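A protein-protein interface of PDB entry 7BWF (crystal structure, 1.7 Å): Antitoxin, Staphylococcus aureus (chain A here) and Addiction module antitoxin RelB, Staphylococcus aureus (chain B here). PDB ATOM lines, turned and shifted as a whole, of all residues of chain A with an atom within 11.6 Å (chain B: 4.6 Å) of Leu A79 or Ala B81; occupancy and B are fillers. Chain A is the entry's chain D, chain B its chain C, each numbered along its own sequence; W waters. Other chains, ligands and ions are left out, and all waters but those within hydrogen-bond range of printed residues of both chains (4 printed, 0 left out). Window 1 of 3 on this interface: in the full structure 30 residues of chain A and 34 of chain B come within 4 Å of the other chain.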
ATOM      1  N   LEU A  62       4.650  -7.869  23.813  1.00  0.00           N
ATOM      2  CA  LEU A  62       4.564  -6.649  23.017  1.00  0.00           C
ATOM      3  C   LEU A  62       5.362  -6.776  21.725  1.00  0.00           C
ATOM      4  O   LEU A  62       4.958  -6.260  20.678  1.00  0.00           O
ATOM      5  CB  LEU A  62       5.057  -5.457  23.842  1.00  0.00           C
ATOM      6  CG  LEU A  62       4.145  -5.030  24.992  1.00  0.00           C
ATOM      7  CD1 LEU A  62       4.903  -4.141  25.968  1.00  0.00           C
ATOM      8  CD2 LEU A  62       2.921  -4.319  24.432  1.00  0.00           C
ATOM      9  N   ASN A  67       4.200  -6.210  13.689  1.00  0.00           N
ATOM     10  CA  ASN A  67       3.560  -4.926  13.426  1.00  0.00           C
ATOM     11  C   ASN A  67       3.458  -4.113  14.706  1.00  0.00           C
ATOM     12  O   ASN A  67       3.724  -2.910  14.708  1.00  0.00           O
ATOM     13  CB  ASN A  67       2.176  -5.125  12.790  1.00  0.00           C
ATOM     14  CG  ASN A  67       2.252  -5.725  11.401  1.00  0.00           C
ATOM     15  OD1 ASN A  67       1.667  -6.774  11.128  1.00  0.00           O
ATOM     16  ND2 ASN A  67       3.006  -5.077  10.524  1.00  0.00           N
ATOM     17  N   ASN A  68       3.108  -4.762  15.816  1.00  0.00           N
ATOM     18  CA  ASN A  68       3.120  -4.053  17.088  1.00  0.00           C
ATOM     19  C   ASN A  68       4.540  -3.644  17.458  1.00  0.00           C
ATOM     20  O   ASN A  68       4.769  -2.529  17.939  1.00  0.00           O
ATOM     21  CB  ASN A  68       2.516  -4.904  18.199  1.00  0.00           C
ATOM     22  CG  ASN A  68       2.147  -4.073  19.410  1.00  0.00           C
ATOM     23  OD1 ASN A  68       1.194  -3.286  19.372  1.00  0.00           O
ATOM     24  ND2 ASN A  68       2.923  -4.205  20.474  1.00  0.00           N
ATOM     25  N   ALA A  69       5.511  -4.528  17.219  1.00  0.00           N
ATOM     26  CA  ALA A  69       6.900  -4.195  17.519  1.00  0.00           C
ATOM     27  C   ALA A  69       7.338  -2.958  16.740  1.00  0.00           C
ATOM     28  O   ALA A  69       8.013  -2.078  17.283  1.00  0.00           O
ATOM     29  CB  ALA A  69       7.813  -5.391  17.214  1.00  0.00           C
ATOM     30  N   GLU A  70       6.947  -2.859  15.468  1.00  0.00           N
ATOM     31  CA  GLU A  70       7.329  -1.695  14.675  1.00  0.00           C
ATOM     32  C   GLU A  70       6.578  -0.452  15.144  1.00  0.00           C
ATOM     33  O   GLU A  70       7.132   0.652  15.160  1.00  0.00           O
ATOM     34  CB  GLU A  70       7.067  -1.969  13.191  1.00  0.00           C
ATOM     35  CG  GLU A  70       7.313  -0.767  12.294  1.00  0.00           C
ATOM     36  CD  GLU A  70       8.789  -0.477  12.093  1.00  0.00           C
ATOM     37  OE1 GLU A  70       9.619  -1.392  12.286  1.00  0.00           O
ATOM     38  OE2 GLU A  70       9.116   0.677  11.749  1.00  0.00           O
ATOM     39  N   HIS A  71       5.317  -0.612  15.538  1.00  0.00           N
ATOM     40  CA  HIS A  71       4.549   0.516  16.056  1.00  0.00           C
ATOM     41  C   HIS A  71       5.179   1.058  17.343  1.00  0.00           C
ATOM     42  O   HIS A  71       5.302   2.275  17.520  1.00  0.00           O
ATOM     43  CB  HIS A  71       3.085   0.072  16.236  1.00  0.00           C
ATOM     44  CG  HIS A  71       2.392   0.701  17.400  1.00  0.00           C
ATOM     45  ND1 HIS A  71       2.053   2.039  17.427  1.00  0.00           N
ATOM     46  CD2 HIS A  71       1.955   0.174  18.569  1.00  0.00           C
ATOM     47  CE1 HIS A  71       1.461   2.313  18.577  1.00  0.00           C
ATOM     48  NE2 HIS A  71       1.385   1.200  19.284  1.00  0.00           N
ATOM     49  N   LEU A  72       5.649   0.171  18.222  1.00  0.00           N
ATOM     50  CA  LEU A  72       6.345   0.607  19.432  1.00  0.00           C
ATOM     51  C   LEU A  72       7.685   1.260  19.101  1.00  0.00           C
ATOM     52  O   LEU A  72       8.022   2.313  19.655  1.00  0.00           O
ATOM     53  CB  LEU A  72       6.556  -0.585  20.371  1.00  0.00           C
ATOM     54  CG  LEU A  72       5.275  -1.134  21.000  1.00  0.00           C
ATOM     55  CD1 LEU A  72       5.577  -2.354  21.868  1.00  0.00           C
ATOM     56  CD2 LEU A  72       4.564  -0.055  21.803  1.00  0.00           C
ATOM     57  N   ALA A  73       8.473   0.647  18.209  1.00  0.00           N
ATOM     58  CA  ALA A  73       9.776   1.211  17.862  1.00  0.00           C
ATOM     59  C   ALA A  73       9.623   2.608  17.273  1.00  0.00           C
ATOM     60  O   ALA A  73      10.296   3.555  17.695  1.00  0.00           O
ATOM     61  CB  ALA A  73      10.514   0.294  16.877  1.00  0.00           C
ATOM     62  N   GLN A  74       8.742   2.758  16.282  1.00  0.00           N
ATOM     63  CA  GLN A  74       8.568   4.062  15.653  1.00  0.00           C
ATOM     64  C   GLN A  74       8.090   5.091  16.670  1.00  0.00           C
ATOM     65  O   GLN A  74       8.546   6.240  16.668  1.00  0.00           O
ATOM     66  CB  GLN A  74       7.577   3.966  14.486  1.00  0.00           C
ATOM     67  CG  GLN A  74       7.226   5.318  13.889  1.00  0.00           C
ATOM     68  CD  GLN A  74       8.344   5.878  13.026  1.00  0.00           C
ATOM     69  OE1 GLN A  74       8.862   5.202  12.134  1.00  0.00           O
ATOM     70  NE2 GLN A  74       8.738   7.115  13.307  1.00  0.00           N
ATOM     71  N   SER A  75       7.162   4.699  17.546  1.00  0.00           N
ATOM     72  CA  SER A  75       6.575   5.657  18.479  1.00  0.00           C
ATOM     73  C   SER A  75       7.598   6.110  19.515  1.00  0.00           C
ATOM     74  O   SER A  75       7.630   7.285  19.889  1.00  0.00           O
ATOM     75  CB  SER A  75       5.345   5.048  19.163  1.00  0.00           C
ATOM     76  OG  SER A  75       4.322   4.785  18.219  1.00  0.00           O
ATOM     77  N   ILE A  76       8.449   5.198  19.986  1.00  0.00           N
ATOM     78  CA  ILE A  76       9.490   5.592  20.930  1.00  0.00           C
ATOM     79  C   ILE A  76      10.547   6.438  20.223  1.00  0.00           C
ATOM     80  O   ILE A  76      11.111   7.367  20.816  1.00  0.00           O
ATOM     81  CB  ILE A  76      10.106   4.353  21.607  1.00  0.00           C
ATOM     82  CG1 ILE A  76       9.058   3.673  22.491  1.00  0.00           C
ATOM     83  CG2 ILE A  76      11.320   4.767  22.427  1.00  0.00           C
ATOM     84  CD1 ILE A  76       9.519   2.362  23.119  1.00  0.00           C
ATOM     85  N   ALA A  77      10.827   6.148  18.952  1.00  0.00           N
ATOM     86  CA  ALA A  77      11.720   7.013  18.186  1.00  0.00           C
ATOM     87  C   ALA A  77      11.100   8.393  17.987  1.00  0.00           C
ATOM     88  O   ALA A  77      11.797   9.409  18.065  1.00  0.00           O
ATOM     89  CB  ALA A  77      12.053   6.371  16.832  1.00  0.00           C
ATOM     90  N   ASP A  78       9.788   8.450  17.738  1.00  0.00           N
ATOM     91  CA  ASP A  78       9.107   9.736  17.611  1.00  0.00           C
ATOM     92  C   ASP A  78       9.225  10.530  18.902  1.00  0.00           C
ATOM     93  O   ASP A  78       9.582  11.711  18.889  1.00  0.00           O
ATOM     94  CB  ASP A  78       7.634   9.520  17.258  1.00  0.00           C
ATOM     95  CG  ASP A  78       7.430   9.111  15.812  1.00  0.00           C
ATOM     96  OD1 ASP A  78       8.385   9.208  15.014  1.00  0.00           O
ATOM     97  OD2 ASP A  78       6.322   8.660  15.479  1.00  0.00           O
ATOM     98  N   LEU A  79       8.941   9.884  20.035  1.00  0.00           N
ATOM     99  CA  LEU A  79       8.964  10.579  21.318  1.00  0.00           C
ATOM    100  C   LEU A  79      10.351  11.138  21.617  1.00  0.00           C
ATOM    101  O   LEU A  79      10.486  12.258  22.119  1.00  0.00           O
ATOM    102  CB  LEU A  79       8.523   9.625  22.434  1.00  0.00           C
ATOM    103  CG  LEU A  79       7.031   9.314  22.559  1.00  0.00           C
ATOM    104  CD1 LEU A  79       6.829   8.129  23.504  1.00  0.00           C
ATOM    105  CD2 LEU A  79       6.275  10.536  23.046  1.00  0.00           C
ATOM    106  N   GLU A  80      11.399  10.373  21.313  1.00  0.00           N
ATOM    107  CA  GLU A  80      12.748  10.840  21.609  1.00  0.00           C
ATOM    108  C   GLU A  80      13.138  12.014  20.721  1.00  0.00           C
ATOM    109  O   GLU A  80      14.001  12.816  21.095  1.00  0.00           O
ATOM    110  CB  GLU A  80      13.751   9.697  21.444  1.00  0.00           C
ATOM    111  CG  GLU A  80      15.078   9.937  22.149  1.00  0.00           C
ATOM    112  CD  GLU A  80      15.905   8.665  22.251  1.00  0.00           C
ATOM    113  OE1 GLU A  80      15.820   7.984  23.292  1.00  0.00           O
ATOM    114  OE2 GLU A  80      16.650   8.354  21.296  1.00  0.00           O
ATOM    115  N   ARG A  81      12.504  12.153  19.558  1.00  0.00           N
ATOM    116  CA  ARG A  81      12.865  13.198  18.608  1.00  0.00           C
ATOM    117  C   ARG A  81      11.967  14.428  18.693  1.00  0.00           C
ATOM    118  O   ARG A  81      12.092  15.331  17.861  1.00  0.00           O
ATOM    119  CB  ARG A  81      12.828  12.642  17.177  1.00  0.00           C
ATOM    120  CG  ARG A  81      14.031  11.785  16.809  1.00  0.00           C
ATOM    121  CD  ARG A  81      13.729  10.791  15.677  1.00  0.00           C
ATOM    122  NE  ARG A  81      14.923  10.003  15.395  1.00  0.00           N
ATOM    123  CZ  ARG A  81      15.441   9.113  16.237  1.00  0.00           C
ATOM    124  NH1 ARG A  81      16.544   8.456  15.908  1.00  0.00           N
ATOM    125  NH2 ARG A  81      14.854   8.872  17.406  1.00  0.00           N
ATOM    126  N   GLY A  82      11.079  14.501  19.677  1.00  0.00           N
ATOM    127  CA  GLY A  82      10.167  15.624  19.729  1.00  0.00           C
ATOM    128  C   GLY A  82       9.044  15.586  18.715  1.00  0.00           C
ATOM    129  O   GLY A  82       8.252  16.533  18.649  1.00  0.00           O
ATOM    130  N   LYS A  83       8.944  14.512  17.932  1.00  0.00           N
ATOM    131  CA  LYS A  83       7.882  14.325  16.939  1.00  0.00           C
ATOM    132  C   LYS A  83       6.614  13.857  17.652  1.00  0.00           C
ATOM    133  O   LYS A  83       6.223  12.691  17.603  1.00  0.00           O
ATOM    134  CB  LYS A  83       8.352  13.318  15.899  1.00  0.00           C
ATOM    135  CG  LYS A  83       7.450  13.034  14.713  1.00  0.00           C
ATOM    136  CD  LYS A  83       8.242  12.127  13.749  1.00  0.00           C
ATOM    137  CE  LYS A  83       7.348  11.183  12.949  1.00  0.00           C
ATOM    138  NZ  LYS A  83       8.084  10.078  12.242  1.00  0.00           N
ATOM    139  N   THR A  84       5.971  14.798  18.343  1.00  0.00           N
ATOM    140  CA  THR A  84       4.935  14.426  19.295  1.00  0.00           C
ATOM    141  C   THR A  84       3.713  15.329  19.223  1.00  0.00           C
ATOM    142  O   THR A  84       3.717  16.408  18.621  1.00  0.00           O
ATOM    143  CB  THR A  84       5.464  14.447  20.739  1.00  0.00           C
ATOM    144  OG1 THR A  84       5.671  15.803  21.150  1.00  0.00           O
ATOM    145  CG2 THR A  84       6.767  13.670  20.834  1.00  0.00           C
ATOM    146  N   ILE A  85       2.665  14.850  19.892  1.00  0.00           N
ATOM    147  CA  ILE A  85       1.438  15.595  20.131  1.00  0.00           C
ATOM    148  C   ILE A  85       1.313  15.808  21.633  1.00  0.00           C
ATOM    149  O   ILE A  85       1.329  14.840  22.408  1.00  0.00           O
ATOM    150  CB  ILE A  85       0.200  14.859  19.601  1.00  0.00           C
ATOM    151  CG1 ILE A  85       0.340  14.508  18.116  1.00  0.00           C
ATOM    152  CG2 ILE A  85      -1.039  15.701  19.821  1.00  0.00           C
ATOM    153  CD1 ILE A  85       0.961  15.596  17.240  1.00  0.00           C
ATOM    154  N   THR A  86       1.171  17.066  22.037  1.00  0.00           N
ATOM    155  CA  THR A  86       0.971  17.439  23.430  1.00  0.00           C
ATOM    156  C   THR A  86      -0.436  17.991  23.613  1.00  0.00           C
ATOM    157  O   THR A  86      -0.803  19.003  23.001  1.00  0.00           O
ATOM    158  CB  THR A  86       2.000  18.469  23.880  1.00  0.00           C
ATOM    159  OG1 THR A  86       3.312  17.931  23.692  1.00  0.00           O
ATOM    160  CG2 THR A  86       1.795  18.795  25.351  1.00  0.00           C
ATOM    161  N   LYS A  87      -1.209  17.323  24.462  1.00  0.00           N
ATOM    162  CA  LYS A  87      -2.589  17.682  24.729  1.00  0.00           C
ATOM    163  C   LYS A  87      -2.829  17.700  26.232  1.00  0.00           C
ATOM    164  O   LYS A  87      -2.368  16.812  26.955  1.00  0.00           O
ATOM    165  CB  LYS A  87      -3.559  16.683  24.077  1.00  0.00           C
ATOM    166  CG  LYS A  87      -3.652  16.753  22.557  1.00  0.00           C
ATOM    167  CD  LYS A  87      -3.959  18.148  22.002  1.00  0.00           C
ATOM    168  CE  LYS A  87      -4.966  18.043  20.854  1.00  0.00           C
ATOM    169  NZ  LYS A  87      -4.706  19.021  19.762  1.00  0.00           N
ATOM    170  N   THR B   6       2.035  13.871  26.765  1.00  0.00           N
ATOM    171  CA  THR B   6       2.696  13.833  25.466  1.00  0.00           C
ATOM    172  C   THR B   6       2.420  12.481  24.821  1.00  0.00           C
ATOM    173  O   THR B   6       2.785  11.438  25.376  1.00  0.00           O
ATOM    174  CB  THR B   6       4.201  14.062  25.591  1.00  0.00           C
ATOM    175  OG1 THR B   6       4.436  15.428  25.952  1.00  0.00           O
ATOM    176  CG2 THR B   6       4.883  13.766  24.277  1.00  0.00           C
ATOM    177  N   PHE B   7       1.768  12.500  23.657  1.00  0.00           N
ATOM    178  CA  PHE B   7       1.514  11.296  22.871  1.00  0.00           C
ATOM    179  C   PHE B   7       2.522  11.154  21.729  1.00  0.00           C
ATOM    180  O   PHE B   7       3.039  12.146  21.215  1.00  0.00           O
ATOM    181  CB  PHE B   7       0.111  11.299  22.227  1.00  0.00           C
ATOM    182  CG  PHE B   7      -1.025  11.309  23.191  1.00  0.00           C
ATOM    183  CD1 PHE B   7      -1.413  12.491  23.779  1.00  0.00           C
ATOM    184  CD2 PHE B   7      -1.741  10.152  23.473  1.00  0.00           C
ATOM    185  CE1 PHE B   7      -2.474  12.531  24.665  1.00  0.00           C
ATOM    186  CE2 PHE B   7      -2.819  10.189  24.362  1.00  0.00           C
ATOM    187  CZ  PHE B   7      -3.174  11.383  24.961  1.00  0.00           C
ATOM    188  N   SER B   8       2.745   9.912  21.287  1.00  0.00           N
ATOM    189  CA  SER B   8       3.358   9.675  19.994  1.00  0.00           C
ATOM    190  C   SER B   8       2.287   9.848  18.929  1.00  0.00           C
ATOM    191  O   SER B   8       1.093   9.659  19.200  1.00  0.00           O
ATOM    192  CB  SER B   8       3.934   8.265  19.921  1.00  0.00           C
ATOM    193  OG  SER B   8       2.913   7.274  19.873  1.00  0.00           O
ATOM    194  N   ALA B  11       0.045   6.684  18.915  1.00  0.00           N
ATOM    195  CA  ALA B  11      -0.679   6.567  20.173  1.00  0.00           C
ATOM    196  C   ALA B  11      -1.818   7.578  20.232  1.00  0.00           C
ATOM    197  O   ALA B  11      -2.913   7.262  20.707  1.00  0.00           O
ATOM    198  CB  ALA B  11       0.287   6.741  21.352  1.00  0.00           C
ATOM    199  N   TYR B  58      10.844   2.159  29.221  1.00  0.00           N
ATOM    200  CA  TYR B  58       9.400   2.292  29.195  1.00  0.00           C
ATOM    201  C   TYR B  58       8.745   1.270  30.108  1.00  0.00           C
ATOM    202  O   TYR B  58       9.378   0.342  30.613  1.00  0.00           O
ATOM    203  CB  TYR B  58       8.872   2.150  27.770  1.00  0.00           C
ATOM    204  CG  TYR B  58       9.098   3.402  26.967  1.00  0.00           C
ATOM    205  CD1 TYR B  58      10.369   3.745  26.528  1.00  0.00           C
ATOM    206  CD2 TYR B  58       8.047   4.257  26.666  1.00  0.00           C
ATOM    207  CE1 TYR B  58      10.583   4.894  25.801  1.00  0.00           C
ATOM    208  CE2 TYR B  58       8.254   5.406  25.938  1.00  0.00           C
ATOM    209  CZ  TYR B  58       9.524   5.722  25.510  1.00  0.00           C
ATOM    210  OH  TYR B  58       9.729   6.871  24.783  1.00  0.00           O
ATOM    211  N   VAL B  70       1.720   1.719  27.072  1.00  0.00           N
ATOM    212  CA  VAL B  70       3.178   1.722  27.072  1.00  0.00           C
ATOM    213  C   VAL B  70       3.644   3.168  27.178  1.00  0.00           C
ATOM    214  O   VAL B  70       3.312   4.004  26.327  1.00  0.00           O
ATOM    215  CB  VAL B  70       3.741   1.053  25.809  1.00  0.00           C
ATOM    216  CG1 VAL B  70       5.249   1.009  25.884  1.00  0.00           C
ATOM    217  CG2 VAL B  70       3.152  -0.347  25.632  1.00  0.00           C
ATOM    218  N   TYR B  71       4.431   3.463  28.212  1.00  0.00           N
ATOM    219  CA  TYR B  71       4.681   4.842  28.593  1.00  0.00           C
ATOM    220  C   TYR B  71       6.014   4.964  29.315  1.00  0.00           C
ATOM    221  O   TYR B  71       6.650   3.976  29.690  1.00  0.00           O
ATOM    222  CB  TYR B  71       3.567   5.362  29.508  1.00  0.00           C
ATOM    223  CG  TYR B  71       3.527   4.609  30.826  1.00  0.00           C
ATOM    224  CD1 TYR B  71       2.817   3.422  30.948  1.00  0.00           C
ATOM    225  CD2 TYR B  71       4.225   5.066  31.938  1.00  0.00           C
ATOM    226  CE1 TYR B  71       2.789   2.721  32.142  1.00  0.00           C
ATOM    227  CE2 TYR B  71       4.198   4.369  33.138  1.00  0.00           C
ATOM    228  CZ  TYR B  71       3.476   3.200  33.236  1.00  0.00           C
ATOM    229  OH  TYR B  71       3.448   2.500  34.422  1.00  0.00           O
ATOM    230  N   LYS B  79       4.739  10.391  29.126  1.00  0.00           N
ATOM    231  CA  LYS B  79       4.809  10.252  27.681  1.00  0.00           C
ATOM    232  C   LYS B  79       4.250   8.895  27.289  1.00  0.00           C
ATOM    233  O   LYS B  79       4.671   7.870  27.838  1.00  0.00           O
ATOM    234  CB  LYS B  79       6.249  10.378  27.192  1.00  0.00           C
ATOM    235  CG  LYS B  79       6.927  11.661  27.625  1.00  0.00           C
ATOM    236  CD  LYS B  79       8.179  11.923  26.795  1.00  0.00           C
ATOM    237  CE  LYS B  79       8.698  13.341  27.004  1.00  0.00           C
ATOM    238  NZ  LYS B  79       9.896  13.667  26.173  1.00  0.00           N
ATOM    239  N   ILE B  80       3.335   8.889  26.322  1.00  0.00           N
ATOM    240  CA  ILE B  80       2.641   7.679  25.900  1.00  0.00           C
ATOM    241  C   ILE B  80       3.191   7.251  24.551  1.00  0.00           C
ATOM    242  O   ILE B  80       3.093   7.990  23.559  1.00  0.00           O
ATOM    243  CB  ILE B  80       1.121   7.893  25.813  1.00  0.00           C
ATOM    244  CG1 ILE B  80       0.557   8.312  27.173  1.00  0.00           C
ATOM    245  CG2 ILE B  80       0.447   6.637  25.332  1.00  0.00           C
ATOM    246  CD1 ILE B  80      -0.953   8.583  27.181  1.00  0.00           C
ATOM    247  N   ALA B  81       3.748   6.045  24.513  1.00  0.00           N
ATOM    248  CA  ALA B  81       4.174   5.449  23.257  1.00  0.00           C
ATOM    249  C   ALA B  81       3.043   4.706  22.551  1.00  0.00           C
ATOM    250  O   ALA B  81       2.979   4.702  21.315  1.00  0.00           O
ATOM    251  CB  ALA B  81       5.346   4.492  23.503  1.00  0.00           C
ATOM    252  N   SER B  82       2.148   4.082  23.312  1.00  0.00           N
ATOM    253  CA  SER B  82       1.109   3.238  22.738  1.00  0.00           C
ATOM    254  C   SER B  82      -0.016   3.092  23.749  1.00  0.00           C
ATOM    255  O   SER B  82       0.211   3.121  24.963  1.00  0.00           O
ATOM    256  CB  SER B  82       1.645   1.848  22.359  1.00  0.00           C
ATOM    257  OG  SER B  82       0.610   1.019  21.854  1.00  0.00           O
HETATM  258  O   HOH W   1       4.000   7.379  16.702  1.00  0.00           O
HETATM  259  O   HOH W   2      -1.081   3.073  20.274  1.00  0.00           O
HETATM  260  O   HOH W   3      11.763   7.603  23.698  1.00  0.00           O
HETATM  261  O   HOH W   4       1.256  -1.890  21.743  1.00  0.00           O
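Hydrophobic or aromatic side chains of chain A within 4 Å of the printed part of chain B: His A71, Leu A72, Ile A76 and Leu A79.
Along chain A the printed residues that touch a printed residue of chain B span positions 71 to 86.
Of the 11 printed residues of chain B, 7 touch a printed residue of chain A.
Printed residues of chain B that touch a printed residue of chain A: Thr B6, Phe B7, Ser B8, Tyr B58, Ile B80, Ala B81 and Ser B82.
Among the printed residues, 17 pairs touch across the chains.
Among the printed residues, no Asp or Glu carboxylate lies within 4 Å of a Lys or Arg side-chain nitrogen of the other chain.
Water W3 bridges OH of Tyr B58 and O of Ile A76.
Water W4 lies within hydrogen-bond range of the side-chain amide oxygen (OD1) of Asn A68 and the side-chain hydroxyl (OG) of Ser B82.
Water W1 lies within hydrogen-bond range of OD2 of Asp A78 (2.9 Å), OG of Ser A75 (3.0 Å) and OG of Ser B8 (3.4 Å).
Water W2 lies within hydrogen-bond range of OG of Ser B82 and NE2 of His A71.
The backbone NH (N) of Phe B7 is in hydrogen-bond range of the backbone carbonyl oxygen (O) of Ile A85 (2.7 Å).
The side-chain hydroxyl (OG) of Ser A75 lies within hydrogen-bond range of the side-chain hydroxyl (OG) of Ser B8 (3.3 Å).
The side-chain hydroxyl (OG) of Ser B82 sits at hydrogen-bond distance from a ring nitrogen (NE2) of His A71, 2.7 Å away.
The side-chain hydroxyl of Ser A75 sits close to the backbone carbonyl oxygen of Ala B81, at 3.4 Å.
Among the printed residues, merely in contact across the chains: His A71 with Ala B81, Leu A72 with Ser B82, Ile A76 with Tyr B58, Ile A76 with Ala B81, Leu A79 with Thr B6, Leu A79 with Ser B8, Leu A79 with Tyr B58, Leu A79 with Ile B80, Leu A79 with Ala B81, Thr A84 with Thr B6, Thr A84 with Phe B7, Ile A85 with Thr B6 and Thr A86 with Thr B6.
The backbone NH of Ala B81 sits at hydrogen-bond distance from the backbone carbonyl oxygen of Val B70 (2.8 Å).
The side-chain hydroxyl of Ser A75 lies within hydrogen-bond range of the backbone carbonyl oxygen of His A71 (2.8 Å).
The side-chain hydroxyl (OG) of Ser B8 sits close to the backbone NH (N) of Ala B11 (3.1 Å).
O of Ala B81 is in hydrogen-bond range of OG of Ser B8.
N of Ser B8 is in hydrogen-bond range of O of Ile B80 (3.0 Å).
The backbone NH (N) of Val B70 lies within hydrogen-bond range of the backbone carbonyl oxygen (O) of Ser B82 (2.9 Å).
Asp A78 touches none of the printed residues of chain B.
Of the printed residues of chain B, Leu A79 touches Thr B6, Ser B8, Tyr B58, Ile B80 and Ala B81.
Arg A81 touches none of the printed residues of chain B.
Of the printed residues of chain A, Thr B6 touches Leu A79 (3.7 Å), Thr A84 (3.6 Å), Ile A85 (3.5 Å) and Thr A86 (3.6 Å).
Of the printed residues of chain A, Ser B8 touches Ser A75 (3.3 Å) and Leu A79 (3.99 Å).
No residue of chain A comes within 4 Å of Ala B11.
Of the printed residues of chain A, Tyr B58 touches Ile A76 and Leu A79.
No residue of chain A comes within 4 Å of Val B70.
No residue of chain A comes within 4 Å of Lys B79.
Of the printed residues of chain A, Ile B80 touches Leu A79.
Printed residues of chain A within 4 Å of Ala B81: His A71 (3.9 Å), Ser A75 (3.2 Å), Ile A76 (3.9 Å) and Leu A79 (3.8 Å).
Ser B82 touches just these residues of chain A: His A71 and Leu A72.
The nearest residue of chain A that does not touch Ala B81 is Leu A72 (4.9 Å).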
